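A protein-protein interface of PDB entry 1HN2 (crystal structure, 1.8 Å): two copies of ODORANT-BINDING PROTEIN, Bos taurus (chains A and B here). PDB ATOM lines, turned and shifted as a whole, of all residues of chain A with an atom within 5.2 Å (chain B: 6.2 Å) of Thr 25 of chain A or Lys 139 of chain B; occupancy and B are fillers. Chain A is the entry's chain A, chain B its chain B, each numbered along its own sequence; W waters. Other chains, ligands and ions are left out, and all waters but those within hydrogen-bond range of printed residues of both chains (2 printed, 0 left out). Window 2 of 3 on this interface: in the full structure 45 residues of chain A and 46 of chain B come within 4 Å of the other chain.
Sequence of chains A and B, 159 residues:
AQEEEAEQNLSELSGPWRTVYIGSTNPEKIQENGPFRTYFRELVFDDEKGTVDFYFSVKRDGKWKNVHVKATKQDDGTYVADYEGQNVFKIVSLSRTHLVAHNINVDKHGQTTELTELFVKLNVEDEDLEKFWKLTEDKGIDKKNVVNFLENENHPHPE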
ATOM      1  N   GLY A  23      34.115  17.940  12.646  1.00  0.00           N
ATOM      2  CA  GLY A  23      33.206  18.596  13.566  1.00  0.00           C
ATOM      3  C   GLY A  23      32.134  17.595  13.968  1.00  0.00           C
ATOM      4  O   GLY A  23      31.899  16.624  13.248  1.00  0.00           O
ATOM      5  N   SER A  24      31.472  17.823  15.099  1.00  0.00           N
ATOM      6  CA  SER A  24      30.446  16.890  15.551  1.00  0.00           C
ATOM      7  C   SER A  24      29.361  17.554  16.393  1.00  0.00           C
ATOM      8  O   SER A  24      29.631  18.489  17.152  1.00  0.00           O
ATOM      9  CB  SER A  24      31.103  15.766  16.360  1.00  0.00           C
ATOM     10  OG  SER A  24      30.145  14.838  16.838  1.00  0.00           O
ATOM     11  N   THR A  25      28.130  17.074  16.245  1.00  0.00           N
ATOM     12  CA  THR A  25      27.020  17.616  17.018  1.00  0.00           C
ATOM     13  C   THR A  25      27.137  17.090  18.445  1.00  0.00           C
ATOM     14  O   THR A  25      26.548  17.640  19.372  1.00  0.00           O
ATOM     15  CB  THR A  25      25.659  17.205  16.416  1.00  0.00           C
ATOM     16  OG1 THR A  25      25.636  15.787  16.206  1.00  0.00           O
ATOM     17  CG2 THR A  25      25.426  17.927  15.090  1.00  0.00           C
ATOM     18  N   ASN A  26      27.908  16.020  18.608  1.00  0.00           N
ATOM     19  CA  ASN A  26      28.151  15.418  19.917  1.00  0.00           C
ATOM     20  C   ASN A  26      29.669  15.420  20.121  1.00  0.00           C
ATOM     21  O   ASN A  26      30.375  14.572  19.571  1.00  0.00           O
ATOM     22  CB  ASN A  26      27.641  13.977  19.958  1.00  0.00           C
ATOM     23  CG  ASN A  26      27.738  13.365  21.343  1.00  0.00           C
ATOM     24  OD1 ASN A  26      28.650  13.677  22.112  1.00  0.00           O
ATOM     25  ND2 ASN A  26      26.800  12.479  21.667  1.00  0.00           N
ATOM     26  N   PRO A  27      30.187  16.367  20.923  1.00  0.00           N
ATOM     27  CA  PRO A  27      31.629  16.475  21.185  1.00  0.00           C
ATOM     28  C   PRO A  27      32.306  15.215  21.727  1.00  0.00           C
ATOM     29  O   PRO A  27      33.483  14.978  21.464  1.00  0.00           O
ATOM     30  CB  PRO A  27      31.714  17.653  22.156  1.00  0.00           C
ATOM     31  CG  PRO A  27      30.419  17.556  22.911  1.00  0.00           C
ATOM     32  CD  PRO A  27      29.427  17.275  21.802  1.00  0.00           C
ATOM     33  N   HIS A 102      29.829  14.883   4.873  1.00  0.00           N
ATOM     34  CA  HIS A 102      28.860  14.949   5.950  1.00  0.00           C
ATOM     35  C   HIS A 102      28.490  13.503   6.289  1.00  0.00           C
ATOM     36  O   HIS A 102      28.107  12.737   5.407  1.00  0.00           O
ATOM     37  CB  HIS A 102      27.623  15.714   5.475  1.00  0.00           C
ATOM     38  CG  HIS A 102      26.457  15.631   6.409  1.00  0.00           C
ATOM     39  ND1 HIS A 102      25.156  15.787   5.980  1.00  0.00           N
ATOM     40  CD2 HIS A 102      26.392  15.423   7.745  1.00  0.00           C
ATOM     41  CE1 HIS A 102      24.339  15.679   7.013  1.00  0.00           C
ATOM     42  NE2 HIS A 102      25.063  15.458   8.096  1.00  0.00           N
ATOM     43  N   THR A 112      21.857   9.627  17.611  1.00  0.00           N
ATOM     44  CA  THR A 112      22.225  10.167  16.311  1.00  0.00           C
ATOM     45  C   THR A 112      23.274  11.278  16.416  1.00  0.00           C
ATOM     46  O   THR A 112      23.114  12.226  17.176  1.00  0.00           O
ATOM     47  CB  THR A 112      20.981  10.727  15.584  1.00  0.00           C
ATOM     48  OG1 THR A 112      20.018   9.681  15.411  1.00  0.00           O
ATOM     49  CG2 THR A 112      21.358  11.283  14.227  1.00  0.00           C
ATOM     50  N   THR A 113      24.346  11.154  15.643  1.00  0.00           N
ATOM     51  CA  THR A 113      25.408  12.154  15.641  1.00  0.00           C
ATOM     52  C   THR A 113      25.732  12.567  14.210  1.00  0.00           C
ATOM     53  O   THR A 113      25.914  11.714  13.341  1.00  0.00           O
ATOM     54  CB  THR A 113      26.710  11.612  16.256  1.00  0.00           C
ATOM     55  OG1 THR A 113      26.459  11.119  17.577  1.00  0.00           O
ATOM     56  CG2 THR A 113      27.765  12.724  16.325  1.00  0.00           C
ATOM     57  N   GLU A 114      25.795  13.868  13.959  1.00  0.00           N
ATOM     58  CA  GLU A 114      26.142  14.333  12.625  1.00  0.00           C
ATOM     59  C   GLU A 114      27.563  14.892  12.674  1.00  0.00           C
ATOM     60  O   GLU A 114      27.921  15.636  13.590  1.00  0.00           O
ATOM     61  CB  GLU A 114      25.154  15.395  12.139  1.00  0.00           C
ATOM     62  CG  GLU A 114      23.723  14.891  12.089  1.00  0.00           C
ATOM     63  CD  GLU A 114      22.852  15.649  11.106  1.00  0.00           C
ATOM     64  OE1 GLU A 114      21.636  15.777  11.367  1.00  0.00           O
ATOM     65  OE2 GLU A 114      23.373  16.104  10.065  1.00  0.00           O
ATOM     66  N   THR A 116      30.968  16.539  10.296  1.00  0.00           N
ATOM     67  CA  THR A 116      31.403  17.185   9.065  1.00  0.00           C
ATOM     68  C   THR A 116      32.910  16.993   9.053  1.00  0.00           C
ATOM     69  O   THR A 116      33.535  16.883  10.105  1.00  0.00           O
ATOM     70  CB  THR A 116      31.106  18.693   9.057  1.00  0.00           C
ATOM     71  OG1 THR A 116      31.717  19.307  10.200  1.00  0.00           O
ATOM     72  CG2 THR A 116      29.600  18.944   9.070  1.00  0.00           C
ATOM     73  N   LYS B 134      30.935  26.331   6.227  1.00  0.00           N
ATOM     74  CA  LYS B 134      29.531  26.572   5.879  1.00  0.00           C
ATOM     75  C   LYS B 134      28.708  25.330   6.187  1.00  0.00           C
ATOM     76  O   LYS B 134      27.635  25.411   6.792  1.00  0.00           O
ATOM     77  CB  LYS B 134      29.414  26.911   4.388  1.00  0.00           C
ATOM     78  CG  LYS B 134      27.983  27.219   3.838  1.00  0.00           C
ATOM     79  CD  LYS B 134      27.215  28.171   4.683  1.00  0.00           C
ATOM     80  CE  LYS B 134      25.825  28.522   4.086  1.00  0.00           C
ATOM     81  NZ  LYS B 134      24.926  27.400   3.687  1.00  0.00           N
ATOM     82  N   LEU B 135      29.204  24.182   5.738  1.00  0.00           N
ATOM     83  CA  LEU B 135      28.526  22.917   5.975  1.00  0.00           C
ATOM     84  C   LEU B 135      28.413  22.687   7.475  1.00  0.00           C
ATOM     85  O   LEU B 135      27.380  22.230   7.974  1.00  0.00           O
ATOM     86  CB  LEU B 135      29.313  21.757   5.344  1.00  0.00           C
ATOM     87  CG  LEU B 135      28.859  20.337   5.716  1.00  0.00           C
ATOM     88  CD1 LEU B 135      27.445  20.088   5.201  1.00  0.00           C
ATOM     89  CD2 LEU B 135      29.829  19.315   5.130  1.00  0.00           C
ATOM     90  N   THR B 136      29.487  23.000   8.193  1.00  0.00           N
ATOM     91  CA  THR B 136      29.515  22.814   9.639  1.00  0.00           C
ATOM     92  C   THR B 136      28.456  23.676  10.324  1.00  0.00           C
ATOM     93  O   THR B 136      27.760  23.217  11.232  1.00  0.00           O
ATOM     94  CB  THR B 136      30.915  23.145  10.205  1.00  0.00           C
ATOM     95  OG1 THR B 136      31.877  22.259   9.618  1.00  0.00           O
ATOM     96  CG2 THR B 136      30.941  22.985  11.731  1.00  0.00           C
ATOM     97  N   GLU B 137      28.318  24.922   9.889  1.00  0.00           N
ATOM     98  CA  GLU B 137      27.315  25.770  10.509  1.00  0.00           C
ATOM     99  C   GLU B 137      25.905  25.403  10.045  1.00  0.00           C
ATOM    100  O   GLU B 137      24.943  25.621  10.775  1.00  0.00           O
ATOM    101  CB  GLU B 137      27.635  27.255  10.282  1.00  0.00           C
ATOM    102  CG  GLU B 137      27.773  27.705   8.896  1.00  0.00           C
ATOM    103  CD  GLU B 137      28.579  28.993   8.806  1.00  0.00           C
ATOM    104  OE1 GLU B 137      28.533  29.670   7.756  1.00  0.00           O
ATOM    105  OE2 GLU B 137      29.270  29.321   9.792  1.00  0.00           O
ATOM    106  N   ASP B 138      25.786  24.819   8.849  1.00  0.00           N
ATOM    107  CA  ASP B 138      24.483  24.390   8.333  1.00  0.00           C
ATOM    108  C   ASP B 138      23.943  23.273   9.230  1.00  0.00           C
ATOM    109  O   ASP B 138      22.732  23.155   9.433  1.00  0.00           O
ATOM    110  CB  ASP B 138      24.586  23.819   6.909  1.00  0.00           C
ATOM    111  CG  ASP B 138      24.670  24.887   5.837  1.00  0.00           C
ATOM    112  OD1 ASP B 138      24.407  26.069   6.130  1.00  0.00           O
ATOM    113  OD2 ASP B 138      24.993  24.531   4.685  1.00  0.00           O
ATOM    114  N   LYS B 139      24.847  22.443   9.745  1.00  0.00           N
ATOM    115  CA  LYS B 139      24.451  21.327  10.596  1.00  0.00           C
ATOM    116  C   LYS B 139      24.340  21.692  12.067  1.00  0.00           C
ATOM    117  O   LYS B 139      24.144  20.824  12.912  1.00  0.00           O
ATOM    118  CB  LYS B 139      25.418  20.154  10.402  1.00  0.00           C
ATOM    119  CG  LYS B 139      25.519  19.724   8.968  1.00  0.00           C
ATOM    120  CD  LYS B 139      24.126  19.481   8.396  1.00  0.00           C
ATOM    121  CE  LYS B 139      24.156  19.067   6.958  1.00  0.00           C
ATOM    122  NZ  LYS B 139      22.774  18.822   6.448  1.00  0.00           N
ATOM    123  N   GLY B 140      24.449  22.982  12.367  1.00  0.00           N
ATOM    124  CA  GLY B 140      24.323  23.429  13.742  1.00  0.00           C
ATOM    125  C   GLY B 140      25.408  22.955  14.690  1.00  0.00           C
ATOM    126  O   GLY B 140      25.153  22.739  15.878  1.00  0.00           O
ATOM    127  N   ILE B 141      26.620  22.791  14.165  1.00  0.00           N
ATOM    128  CA  ILE B 141      27.758  22.354  14.968  1.00  0.00           C
ATOM    129  C   ILE B 141      28.521  23.571  15.480  1.00  0.00           C
ATOM    130  O   ILE B 141      28.916  24.443  14.706  1.00  0.00           O
ATOM    131  CB  ILE B 141      28.705  21.449  14.136  1.00  0.00           C
ATOM    132  CG1 ILE B 141      27.987  20.139  13.799  1.00  0.00           C
ATOM    133  CG2 ILE B 141      29.996  21.171  14.904  1.00  0.00           C
ATOM    134  CD1 ILE B 141      28.756  19.232  12.831  1.00  0.00           C
ATOM    135  N   ASN B 145      33.284  22.629  18.942  1.00  0.00           N
ATOM    136  CA  ASN B 145      33.089  21.199  18.784  1.00  0.00           C
ATOM    137  C   ASN B 145      33.749  20.714  17.493  1.00  0.00           C
ATOM    138  O   ASN B 145      33.272  19.784  16.844  1.00  0.00           O
ATOM    139  CB  ASN B 145      31.595  20.880  18.775  1.00  0.00           C
ATOM    140  CG  ASN B 145      30.984  20.935  20.165  1.00  0.00           C
ATOM    141  OD1 ASN B 145      29.766  21.002  20.319  1.00  0.00           O
ATOM    142  ND2 ASN B 145      31.834  20.890  21.187  1.00  0.00           N
HETATM  143  O   HOH W   1      28.374  20.605  18.206  1.00  0.00           O
HETATM  144  O   HOH W   2      21.636  16.910   8.213  1.00  0.00           O
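The side-chain hydroxyl (OG1) of Thr 116 of chain A lies within hydrogen-bond range of the side-chain hydroxyl (OG1) of Thr 136 of chain B (3.0 Å).
N of Ser 24 of chain A sits at hydrogen-bond distance from O of Asn 145 of chain B, 3.2 Å away.
Of the 10 printed residues of chain A, 7 touch a printed residue of chain B.
Hydrophobic or aromatic side chains of chain A within 4 Å of the printed part of chain B: Pro 27 and His 102.
Among the printed residues, no Asp or Glu carboxylate lies within 4 Å of a Lys or Arg side-chain nitrogen of the other chain.
The side-chain carboxylate (OE2) of Glu 114 of chain A is in hydrogen-bond range of a ring nitrogen (NE2) of His 102 of chain A (2.7 Å).
The backbone carbonyl oxygen (O) of Asn 26 of chain A is in hydrogen-bond range of the side-chain hydroxyl (OG) of Ser 24 of chain A (2.8 Å).
OG1 of Thr 25 of chain A lies within hydrogen-bond range of N of Glu 114 of chain A (3.0 Å).
The backbone NH (N) of Ile 141 of chain B lies within hydrogen-bond range of the backbone carbonyl oxygen (O) of Thr 136 of chain B (3.2 Å).
O of Thr 116 of chain A is in hydrogen-bond range of N of Gly 23 of chain A (2.8 Å).
Water W1 lies within hydrogen-bond range of the side-chain amide oxygen of Asn 145 of chain B (2.6 Å) and the backbone carbonyl oxygen of Ser 24 of chain A (2.7 Å).
Water W2 lies within hydrogen-bond range of the side-chain carboxylate of Glu 114 of chain A (2.7 Å) and the side-chain amino group of Lys 139 of chain B (2.8 Å).
Of the printed residues of chain B, Thr 25 of chain A touches Lys 139 (3.8 Å) and Ile 141 (3.6 Å).
Lys 139 of chain B touches just these residues of chain A: Thr 25, His 102 and Glu 114.
Of the printed residues of chain B, Thr 116 of chain A touches Leu 135, Thr 136 and Ile 141.
Of the printed residues of chain A, Asn 145 of chain B touches Gly 23, Ser 24 and Pro 27.
Asp 138 of chain B touches none of the printed residues of chain A.
The nearest residue of chain B that does not touch Thr 25 of chain A is Asn 145 of chain B (4.7 Å).
No position is printed for both chains.
Of the 13 pairs that touch across the chains among the printed residues, none has its exchanged pair printed and touching as well.
Among the printed residues, pairs that only touch across the chains: Gly 23 of chain A with Ile 141 of chain B (3.9 Å), Gly 23 of chain A with Asn 145 of chain B (3.5 Å), Ser 24 of chain A with Ile 141 of chain B (3.5 Å), Thr 25 of chain A with Lys 139 of chain B (3.8 Å), Thr 25 of chain A with Ile 141 of chain B (3.6 Å), Pro 27 of chain A with Asn 145 of chain B (3.4 Å), His 102 of chain A with Lys 139 of chain B (3.4 Å), Glu 114 of chain A with Lys 139 of chain B (3.8 Å), Glu 114 of chain A with Ile 141 of chain B (3.8 Å), Thr 116 of chain A with Leu 135 of chain B (3.7 Å) and Thr 116 of chain A with Ile 141 of chain B (3.9 Å).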
